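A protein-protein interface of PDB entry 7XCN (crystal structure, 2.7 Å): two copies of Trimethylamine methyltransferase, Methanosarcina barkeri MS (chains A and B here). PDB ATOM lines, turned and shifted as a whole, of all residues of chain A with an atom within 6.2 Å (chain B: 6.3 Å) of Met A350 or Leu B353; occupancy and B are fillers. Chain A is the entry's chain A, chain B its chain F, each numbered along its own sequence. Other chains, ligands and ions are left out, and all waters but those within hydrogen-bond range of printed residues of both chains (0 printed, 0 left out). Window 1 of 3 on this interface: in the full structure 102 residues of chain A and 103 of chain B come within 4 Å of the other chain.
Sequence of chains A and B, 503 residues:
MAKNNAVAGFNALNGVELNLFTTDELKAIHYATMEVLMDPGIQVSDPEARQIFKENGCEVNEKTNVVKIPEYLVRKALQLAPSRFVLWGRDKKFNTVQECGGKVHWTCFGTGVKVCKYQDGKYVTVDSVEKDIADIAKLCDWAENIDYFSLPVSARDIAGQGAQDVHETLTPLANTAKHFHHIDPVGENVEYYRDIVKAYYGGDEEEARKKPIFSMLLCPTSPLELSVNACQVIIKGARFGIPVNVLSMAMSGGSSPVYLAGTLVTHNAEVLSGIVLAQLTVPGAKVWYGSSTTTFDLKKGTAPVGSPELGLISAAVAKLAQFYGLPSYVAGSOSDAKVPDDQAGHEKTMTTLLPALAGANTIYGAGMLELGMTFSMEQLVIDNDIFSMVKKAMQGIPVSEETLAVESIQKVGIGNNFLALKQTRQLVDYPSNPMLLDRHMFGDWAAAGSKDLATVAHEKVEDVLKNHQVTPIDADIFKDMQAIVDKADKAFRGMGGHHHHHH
Of the printed residues of chain A, Leu B353 touches Met A350. Printed residues of chain B within 4 Å of Pro A308: Met B389 (3.4 Å) and Ala B393 (3.96 Å). Of the printed residues of chain B, His A346 touches Thr B349 (2.7 Å) and Met B389 (3.9 Å). The nearest printed residue of chain A that does not touch Leu B353 is Leu A353 (4.01 Å). The nearest printed residue of chain B that does not touch Leu A353 is Leu B353 (4.01 Å).
CB of Pro A308 touches O of Met B389 (3.4 Å). CB of Ala B393 touches CB of Pro A308, at 3.96 Å. His A346 touches Met B389 (NE2 to CG, 3.9 Å). CG2 of Thr B349 touches CG2 of Thr A349, 3.8 Å away. N of Met B350 touches CG2 of Thr A349, at 3.9 Å. Met A350 touches Thr B349 (N to CG2, 3.9 Å). Met A350 touches Leu B353. CE of Met A350 touches CB of Ala B393, at 3.9 Å. CE of Met B350 touches CD2 of Leu A353 (3.5 Å).
ND1 of His A346 lies within hydrogen-bond range of OG1 of Thr B349 (2.7 Å).
Of the 18 printed residues of chain B, 5 touch a printed residue of chain A. Along chain B the printed residues that touch a printed residue of chain A span positions 349 to 393. Of the 16 printed residues of chain A, 5 touch a printed residue of chain B. Along chain A the printed residues that touch a printed residue of chain B span positions 308 to 353. Among the printed residues, no Asp or Glu carboxylate lies within 4 Å of a Lys or Arg side-chain nitrogen of the other chain.
The side-chain hydroxyl (OG1) of Thr A349 sits at hydrogen-bond distance from the backbone carbonyl oxygen (O) of Gly A345 (2.9 Å).
Thr B349 touches its own counterpart, Thr A349. Thr A349 touches Met B350, and with the chains exchanged Met A350 touches Thr B349. Met A350 touches Leu B353, and with the chains exchanged Leu A353 touches Met B350. 9 positions are printed for both chains.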
ATOM      1  N   GLY A 306       0.373   7.721  -3.968  1.00  0.00           N
ATOM      2  CA  GLY A 306      -0.926   8.363  -4.005  1.00  0.00           C
ATOM      3  C   GLY A 306      -1.444   8.548  -2.597  1.00  0.00           C
ATOM      4  O   GLY A 306      -2.612   8.865  -2.387  1.00  0.00           O
ATOM      5  N   SER A 307      -0.563   8.354  -1.623  1.00  0.00           N
ATOM      6  CA  SER A 307      -0.934   8.485  -0.222  1.00  0.00           C
ATOM      7  C   SER A 307      -1.036   9.943   0.175  1.00  0.00           C
ATOM      8  O   SER A 307      -0.606  10.827  -0.560  1.00  0.00           O
ATOM      9  CB  SER A 307       0.114   7.821   0.675  1.00  0.00           C
ATOM     10  OG  SER A 307       1.317   8.574   0.688  1.00  0.00           O
ATOM     11  N   PRO A 308      -1.624  10.213   1.348  1.00  0.00           N
ATOM     12  CA  PRO A 308      -1.731  11.604   1.783  1.00  0.00           C
ATOM     13  C   PRO A 308      -0.329  12.105   2.160  1.00  0.00           C
ATOM     14  O   PRO A 308      -0.086  13.301   2.263  1.00  0.00           O
ATOM     15  CB  PRO A 308      -2.686  11.515   2.973  1.00  0.00           C
ATOM     16  CG  PRO A 308      -2.432  10.140   3.514  1.00  0.00           C
ATOM     17  CD  PRO A 308      -2.350   9.316   2.265  1.00  0.00           C
ATOM     18  N   GLY A 311       1.225  13.785  -0.804  1.00  0.00           N
ATOM     19  CA  GLY A 311       0.552  15.066  -0.915  1.00  0.00           C
ATOM     20  C   GLY A 311       1.161  16.089   0.029  1.00  0.00           C
ATOM     21  O   GLY A 311       1.378  17.245  -0.358  1.00  0.00           O
ATOM     22  N   GLY A 345      -9.411   8.501  -8.721  1.00  0.00           N
ATOM     23  CA  GLY A 345      -9.936   9.837  -8.522  1.00  0.00           C
ATOM     24  C   GLY A 345      -9.614  10.410  -7.157  1.00  0.00           C
ATOM     25  O   GLY A 345      -9.181  11.556  -7.050  1.00  0.00           O
ATOM     26  N   HIS A 346      -9.827   9.624  -6.107  1.00  0.00           N
ATOM     27  CA  HIS A 346      -9.537  10.081  -4.744  1.00  0.00           C
ATOM     28  C   HIS A 346      -8.064  10.450  -4.564  1.00  0.00           C
ATOM     29  O   HIS A 346      -7.739  11.579  -4.198  1.00  0.00           O
ATOM     30  CB  HIS A 346      -9.908   9.001  -3.726  1.00  0.00           C
ATOM     31  CG  HIS A 346      -9.128   9.085  -2.453  1.00  0.00           C
ATOM     32  ND1 HIS A 346      -9.183  10.176  -1.618  1.00  0.00           N
ATOM     33  CD2 HIS A 346      -8.254   8.220  -1.886  1.00  0.00           C
ATOM     34  CE1 HIS A 346      -8.375   9.984  -0.591  1.00  0.00           C
ATOM     35  NE2 HIS A 346      -7.799   8.804  -0.729  1.00  0.00           N
ATOM     36  N   GLU A 347      -7.178   9.490  -4.819  1.00  0.00           N
ATOM     37  CA  GLU A 347      -5.750   9.720  -4.672  1.00  0.00           C
ATOM     38  C   GLU A 347      -5.282  10.850  -5.593  1.00  0.00           C
ATOM     39  O   GLU A 347      -4.548  11.744  -5.167  1.00  0.00           O
ATOM     40  CB  GLU A 347      -4.980   8.407  -4.910  1.00  0.00           C
ATOM     41  CG  GLU A 347      -5.345   7.320  -3.868  1.00  0.00           C
ATOM     42  CD  GLU A 347      -4.510   6.031  -3.953  1.00  0.00           C
ATOM     43  OE1 GLU A 347      -4.388   5.466  -5.061  1.00  0.00           O
ATOM     44  OE2 GLU A 347      -3.990   5.571  -2.904  1.00  0.00           O
ATOM     45  N   LYS A 348      -5.728  10.837  -6.841  1.00  0.00           N
ATOM     46  CA  LYS A 348      -5.338  11.886  -7.780  1.00  0.00           C
ATOM     47  C   LYS A 348      -5.657  13.255  -7.212  1.00  0.00           C
ATOM     48  O   LYS A 348      -4.897  14.192  -7.398  1.00  0.00           O
ATOM     49  CB  LYS A 348      -6.083  11.744  -9.109  1.00  0.00           C
ATOM     50  CG  LYS A 348      -5.609  10.619 -10.005  1.00  0.00           C
ATOM     51  CD  LYS A 348      -4.268  10.936 -10.602  1.00  0.00           C
ATOM     52  CE  LYS A 348      -3.888   9.886 -11.612  1.00  0.00           C
ATOM     53  NZ  LYS A 348      -2.619  10.241 -12.285  1.00  0.00           N
ATOM     54  N   THR A 349      -6.790  13.361  -6.524  1.00  0.00           N
ATOM     55  CA  THR A 349      -7.235  14.627  -5.954  1.00  0.00           C
ATOM     56  C   THR A 349      -6.508  15.003  -4.667  1.00  0.00           C
ATOM     57  O   THR A 349      -6.142  16.153  -4.469  1.00  0.00           O
ATOM     58  CB  THR A 349      -8.753  14.587  -5.690  1.00  0.00           C
ATOM     59  OG1 THR A 349      -9.446  14.487  -6.939  1.00  0.00           O
ATOM     60  CG2 THR A 349      -9.211  15.844  -4.951  1.00  0.00           C
ATOM     61  N   MET A 350      -6.320  14.021  -3.798  1.00  0.00           N
ATOM     62  CA  MET A 350      -5.639  14.205  -2.524  1.00  0.00           C
ATOM     63  C   MET A 350      -4.218  14.703  -2.743  1.00  0.00           C
ATOM     64  O   MET A 350      -3.803  15.695  -2.145  1.00  0.00           O
ATOM     65  CB  MET A 350      -5.586  12.873  -1.781  1.00  0.00           C
ATOM     66  CG  MET A 350      -4.605  12.822  -0.636  1.00  0.00           C
ATOM     67  SD  MET A 350      -5.337  13.471   0.853  1.00  0.00           S
ATOM     68  CE  MET A 350      -4.790  15.134   0.772  1.00  0.00           C
ATOM     69  N   THR A 351      -3.486  13.999  -3.607  1.00  0.00           N
ATOM     70  CA  THR A 351      -2.098  14.328  -3.902  1.00  0.00           C
ATOM     71  C   THR A 351      -1.911  15.546  -4.805  1.00  0.00           C
ATOM     72  O   THR A 351      -0.784  15.972  -5.042  1.00  0.00           O
ATOM     73  CB  THR A 351      -1.354  13.116  -4.534  1.00  0.00           C
ATOM     74  OG1 THR A 351      -1.828  12.882  -5.866  1.00  0.00           O
ATOM     75  CG2 THR A 351      -1.586  11.869  -3.708  1.00  0.00           C
ATOM     76  N   THR A 352      -2.996  16.116  -5.313  1.00  0.00           N
ATOM     77  CA  THR A 352      -2.856  17.294  -6.166  1.00  0.00           C
ATOM     78  C   THR A 352      -3.347  18.551  -5.449  1.00  0.00           C
ATOM     79  O   THR A 352      -2.752  19.629  -5.572  1.00  0.00           O
ATOM     80  CB  THR A 352      -3.634  17.145  -7.501  1.00  0.00           C
ATOM     81  OG1 THR A 352      -3.458  18.323  -8.295  1.00  0.00           O
ATOM     82  CG2 THR A 352      -5.111  16.972  -7.241  1.00  0.00           C
ATOM     83  N   LEU A 353      -4.423  18.405  -4.684  1.00  0.00           N
ATOM     84  CA  LEU A 353      -4.998  19.537  -3.980  1.00  0.00           C
ATOM     85  C   LEU A 353      -4.040  20.152  -2.964  1.00  0.00           C
ATOM     86  O   LEU A 353      -3.929  21.376  -2.878  1.00  0.00           O
ATOM     87  CB  LEU A 353      -6.306  19.116  -3.313  1.00  0.00           C
ATOM     88  CG  LEU A 353      -7.266  20.217  -2.857  1.00  0.00           C
ATOM     89  CD1 LEU A 353      -7.251  21.406  -3.818  1.00  0.00           C
ATOM     90  CD2 LEU A 353      -8.655  19.607  -2.757  1.00  0.00           C
ATOM     91  N   LEU A 354      -3.332  19.311  -2.212  1.00  0.00           N
ATOM     92  CA  LEU A 354      -2.384  19.812  -1.222  1.00  0.00           C
ATOM     93  C   LEU A 354      -1.286  20.671  -1.830  1.00  0.00           C
ATOM     94  O   LEU A 354      -1.180  21.845  -1.497  1.00  0.00           O
ATOM     95  CB  LEU A 354      -1.763  18.664  -0.432  1.00  0.00           C
ATOM     96  CG  LEU A 354      -2.767  17.895   0.423  1.00  0.00           C
ATOM     97  CD1 LEU A 354      -2.026  16.946   1.358  1.00  0.00           C
ATOM     98  CD2 LEU A 354      -3.618  18.880   1.214  1.00  0.00           C
ATOM     99  N   PRO A 355      -0.452  20.110  -2.726  1.00  0.00           N
ATOM    100  CA  PRO A 355       0.604  20.946  -3.307  1.00  0.00           C
ATOM    101  C   PRO A 355       0.061  22.114  -4.131  1.00  0.00           C
ATOM    102  O   PRO A 355       0.746  23.121  -4.316  1.00  0.00           O
ATOM    103  CB  PRO A 355       1.415  19.956  -4.138  1.00  0.00           C
ATOM    104  CG  PRO A 355       0.413  18.941  -4.530  1.00  0.00           C
ATOM    105  CD  PRO A 355      -0.385  18.743  -3.266  1.00  0.00           C
ATOM    106  N   LEU A 357      -2.792  23.955  -3.367  1.00  0.00           N
ATOM    107  CA  LEU A 357      -3.146  24.978  -2.380  1.00  0.00           C
ATOM    108  C   LEU A 357      -1.887  25.529  -1.722  1.00  0.00           C
ATOM    109  O   LEU A 357      -1.850  26.672  -1.266  1.00  0.00           O
ATOM    110  CB  LEU A 357      -4.106  24.394  -1.322  1.00  0.00           C
ATOM    111  CG  LEU A 357      -5.380  23.759  -1.933  1.00  0.00           C
ATOM    112  CD1 LEU A 357      -6.151  22.907  -0.912  1.00  0.00           C
ATOM    113  CD2 LEU A 357      -6.262  24.869  -2.511  1.00  0.00           C
ATOM    114  N   LEU B  18      -5.743  26.157   6.749  1.00  0.00           N
ATOM    115  CA  LEU B  18      -6.268  26.620   5.472  1.00  0.00           C
ATOM    116  C   LEU B  18      -6.998  27.932   5.706  1.00  0.00           C
ATOM    117  O   LEU B  18      -7.851  28.022   6.581  1.00  0.00           O
ATOM    118  CB  LEU B  18      -7.215  25.575   4.872  1.00  0.00           C
ATOM    119  CG  LEU B  18      -7.786  25.895   3.490  1.00  0.00           C
ATOM    120  CD1 LEU B  18      -8.009  24.623   2.716  1.00  0.00           C
ATOM    121  CD2 LEU B  18      -9.083  26.673   3.642  1.00  0.00           C
ATOM    122  N   SER B 333     -17.641  15.344   1.305  1.00  0.00           N
ATOM    123  CA  SER B 333     -17.605  13.973   0.805  1.00  0.00           C
ATOM    124  C   SER B 333     -18.901  13.682   0.047  1.00  0.00           C
ATOM    125  O   SER B 333     -19.574  12.690   0.298  1.00  0.00           O
ATOM    126  CB  SER B 333     -17.409  12.967   1.950  1.00  0.00           C
ATOM    127  OG  SER B 333     -18.442  13.053   2.914  1.00  0.00           O
ATOM    128  N   LYS B 348     -15.724  13.359  -4.049  1.00  0.00           N
ATOM    129  CA  LYS B 348     -15.783  13.058  -2.624  1.00  0.00           C
ATOM    130  C   LYS B 348     -14.586  13.640  -1.871  1.00  0.00           C
ATOM    131  O   LYS B 348     -14.734  14.167  -0.767  1.00  0.00           O
ATOM    132  CB  LYS B 348     -15.824  11.546  -2.395  1.00  0.00           C
ATOM    133  CG  LYS B 348     -17.104  10.866  -2.834  1.00  0.00           C
ATOM    134  CD  LYS B 348     -18.213  11.142  -1.865  1.00  0.00           C
ATOM    135  CE  LYS B 348     -19.433  10.323  -2.194  1.00  0.00           C
ATOM    136  NZ  LYS B 348     -20.400  10.374  -1.079  1.00  0.00           N
ATOM    137  N   THR B 349     -13.405  13.546  -2.474  1.00  0.00           N
ATOM    138  CA  THR B 349     -12.184  14.035  -1.844  1.00  0.00           C
ATOM    139  C   THR B 349     -12.066  15.549  -1.898  1.00  0.00           C
ATOM    140  O   THR B 349     -11.545  16.177  -0.979  1.00  0.00           O
ATOM    141  CB  THR B 349     -10.938  13.415  -2.501  1.00  0.00           C
ATOM    142  OG1 THR B 349     -11.051  11.990  -2.476  1.00  0.00           O
ATOM    143  CG2 THR B 349      -9.683  13.813  -1.743  1.00  0.00           C
ATOM    144  N   MET B 350     -12.544  16.134  -2.987  1.00  0.00           N
ATOM    145  CA  MET B 350     -12.498  17.578  -3.154  1.00  0.00           C
ATOM    146  C   MET B 350     -13.407  18.259  -2.128  1.00  0.00           C
ATOM    147  O   MET B 350     -12.986  19.169  -1.422  1.00  0.00           O
ATOM    148  CB  MET B 350     -12.950  17.938  -4.572  1.00  0.00           C
ATOM    149  CG  MET B 350     -13.248  19.422  -4.808  1.00  0.00           C
ATOM    150  SD  MET B 350     -11.887  20.347  -5.558  1.00  0.00           S
ATOM    151  CE  MET B 350     -11.342  21.308  -4.180  1.00  0.00           C
ATOM    152  N   THR B 351     -14.651  17.797  -2.045  1.00  0.00           N
ATOM    153  CA  THR B 351     -15.626  18.391  -1.144  1.00  0.00           C
ATOM    154  C   THR B 351     -15.421  18.022   0.306  1.00  0.00           C
ATOM    155  O   THR B 351     -16.128  18.520   1.173  1.00  0.00           O
ATOM    156  CB  THR B 351     -17.059  17.998  -1.521  1.00  0.00           C
ATOM    157  OG1 THR B 351     -17.205  16.580  -1.404  1.00  0.00           O
ATOM    158  CG2 THR B 351     -17.376  18.431  -2.945  1.00  0.00           C
ATOM    159  N   THR B 352     -14.470  17.141   0.584  1.00  0.00           N
ATOM    160  CA  THR B 352     -14.242  16.774   1.968  1.00  0.00           C
ATOM    161  C   THR B 352     -12.957  17.422   2.486  1.00  0.00           C
ATOM    162  O   THR B 352     -12.907  17.945   3.605  1.00  0.00           O
ATOM    163  CB  THR B 352     -14.188  15.226   2.142  1.00  0.00           C
ATOM    164  OG1 THR B 352     -14.064  14.901   3.526  1.00  0.00           O
ATOM    165  CG2 THR B 352     -13.014  14.643   1.421  1.00  0.00           C
ATOM    166  N   LEU B 353     -11.929  17.414   1.650  1.00  0.00           N
ATOM    167  CA  LEU B 353     -10.631  17.976   2.006  1.00  0.00           C
ATOM    168  C   LEU B 353     -10.688  19.455   2.399  1.00  0.00           C
ATOM    169  O   LEU B 353     -10.113  19.849   3.417  1.00  0.00           O
ATOM    170  CB  LEU B 353      -9.664  17.774   0.841  1.00  0.00           C
ATOM    171  CG  LEU B 353      -8.187  17.628   1.178  1.00  0.00           C
ATOM    172  CD1 LEU B 353      -7.968  16.834   2.468  1.00  0.00           C
ATOM    173  CD2 LEU B 353      -7.547  16.920   0.005  1.00  0.00           C
ATOM    174  N   LEU B 354     -11.375  20.268   1.597  1.00  0.00           N
ATOM    175  CA  LEU B 354     -11.492  21.684   1.902  1.00  0.00           C
ATOM    176  C   LEU B 354     -12.149  21.940   3.264  1.00  0.00           C
ATOM    177  O   LEU B 354     -11.521  22.524   4.145  1.00  0.00           O
ATOM    178  CB  LEU B 354     -12.272  22.403   0.807  1.00  0.00           C
ATOM    179  CG  LEU B 354     -11.558  22.437  -0.534  1.00  0.00           C
ATOM    180  CD1 LEU B 354     -12.474  22.999  -1.612  1.00  0.00           C
ATOM    181  CD2 LEU B 354     -10.316  23.275  -0.391  1.00  0.00           C
ATOM    182  N   PRO B 355     -13.408  21.499   3.467  1.00  0.00           N
ATOM    183  CA  PRO B 355     -14.019  21.758   4.777  1.00  0.00           C
ATOM    184  C   PRO B 355     -13.265  21.133   5.961  1.00  0.00           C
ATOM    185  O   PRO B 355     -13.302  21.656   7.075  1.00  0.00           O
ATOM    186  CB  PRO B 355     -15.447  21.218   4.609  1.00  0.00           C
ATOM    187  CG  PRO B 355     -15.286  20.128   3.594  1.00  0.00           C
ATOM    188  CD  PRO B 355     -14.327  20.743   2.595  1.00  0.00           C
ATOM    189  N   ALA B 356     -12.580  20.019   5.724  1.00  0.00           N
ATOM    190  CA  ALA B 356     -11.825  19.372   6.793  1.00  0.00           C
ATOM    191  C   ALA B 356     -10.622  20.242   7.147  1.00  0.00           C
ATOM    192  O   ALA B 356     -10.419  20.587   8.315  1.00  0.00           O
ATOM    193  CB  ALA B 356     -11.364  17.990   6.355  1.00  0.00           C
ATOM    194  N   LEU B 357      -9.825  20.596   6.140  1.00  0.00           N
ATOM    195  CA  LEU B 357      -8.672  21.456   6.378  1.00  0.00           C
ATOM    196  C   LEU B 357      -9.129  22.783   6.990  1.00  0.00           C
ATOM    197  O   LEU B 357      -8.374  23.432   7.711  1.00  0.00           O
ATOM    198  CB  LEU B 357      -7.909  21.708   5.070  1.00  0.00           C
ATOM    199  CG  LEU B 357      -7.289  20.430   4.483  1.00  0.00           C
ATOM    200  CD1 LEU B 357      -6.630  20.727   3.154  1.00  0.00           C
ATOM    201  CD2 LEU B 357      -6.282  19.836   5.471  1.00  0.00           C
ATOM    202  N   ALA B 358     -10.378  23.160   6.723  1.00  0.00           N
ATOM    203  CA  ALA B 358     -10.935  24.409   7.233  1.00  0.00           C
ATOM    204  C   ALA B 358     -11.398  24.302   8.680  1.00  0.00           C
ATOM    205  O   ALA B 358     -11.516  25.314   9.378  1.00  0.00           O
ATOM    206  CB  ALA B 358     -12.089  24.858   6.352  1.00  0.00           C
ATOM    207  N   ILE B 363     -18.922  16.990   9.054  1.00  0.00           N
ATOM    208  CA  ILE B 363     -18.967  17.014   7.604  1.00  0.00           C
ATOM    209  C   ILE B 363     -19.858  15.860   7.226  1.00  0.00           C
ATOM    210  O   ILE B 363     -19.517  14.701   7.484  1.00  0.00           O
ATOM    211  CB  ILE B 363     -17.577  16.789   6.985  1.00  0.00           C
ATOM    212  CG1 ILE B 363     -16.630  17.924   7.395  1.00  0.00           C
ATOM    213  CG2 ILE B 363     -17.702  16.706   5.478  1.00  0.00           C
ATOM    214  CD1 ILE B 363     -15.211  17.723   6.932  1.00  0.00           C
ATOM    215  N   MET B 389      -7.451   8.627   5.345  1.00  0.00           N
ATOM    216  CA  MET B 389      -6.397   9.280   4.581  1.00  0.00           C
ATOM    217  C   MET B 389      -6.424  10.777   4.854  1.00  0.00           C
ATOM    218  O   MET B 389      -5.376  11.402   5.025  1.00  0.00           O
ATOM    219  CB  MET B 389      -6.580   9.023   3.084  1.00  0.00           C
ATOM    220  CG  MET B 389      -6.563   7.557   2.704  1.00  0.00           C
ATOM    221  SD  MET B 389      -5.078   6.686   3.278  1.00  0.00           S
ATOM    222  CE  MET B 389      -5.649   6.058   4.894  1.00  0.00           C
ATOM    223  N   VAL B 390      -7.621  11.351   4.898  1.00  0.00           N
ATOM    224  CA  VAL B 390      -7.752  12.775   5.170  1.00  0.00           C
ATOM    225  C   VAL B 390      -7.247  13.105   6.575  1.00  0.00           C
ATOM    226  O   VAL B 390      -6.592  14.135   6.778  1.00  0.00           O
ATOM    227  CB  VAL B 390      -9.218  13.237   5.039  1.00  0.00           C
ATOM    228  CG1 VAL B 390      -9.352  14.686   5.492  1.00  0.00           C
ATOM    229  CG2 VAL B 390      -9.673  13.096   3.592  1.00  0.00           C
ATOM    230  N   ALA B 393      -3.556  13.324   6.441  1.00  0.00           N
ATOM    231  CA  ALA B 393      -3.120  14.563   5.822  1.00  0.00           C
ATOM    232  C   ALA B 393      -3.212  15.689   6.837  1.00  0.00           C
ATOM    233  O   ALA B 393      -2.336  16.548   6.891  1.00  0.00           O
ATOM    234  CB  ALA B 393      -3.977  14.871   4.624  1.00  0.00           C
ATOM    235  N   MET B 394      -4.269  15.670   7.652  1.00  0.00           N
ATOM    236  CA  MET B 394      -4.473  16.699   8.666  1.00  0.00           C
ATOM    237  C   MET B 394      -3.435  16.739   9.793  1.00  0.00           C
ATOM    238  O   MET B 394      -3.403  17.692  10.575  1.00  0.00           O
ATOM    239  CB  MET B 394      -5.868  16.577   9.262  1.00  0.00           C
ATOM    240  CG  MET B 394      -6.948  17.191   8.410  1.00  0.00           C
ATOM    241  SD  MET B 394      -8.566  16.889   9.100  1.00  0.00           S
ATOM    242  CE  MET B 394      -8.597  18.009  10.504  1.00  0.00           C
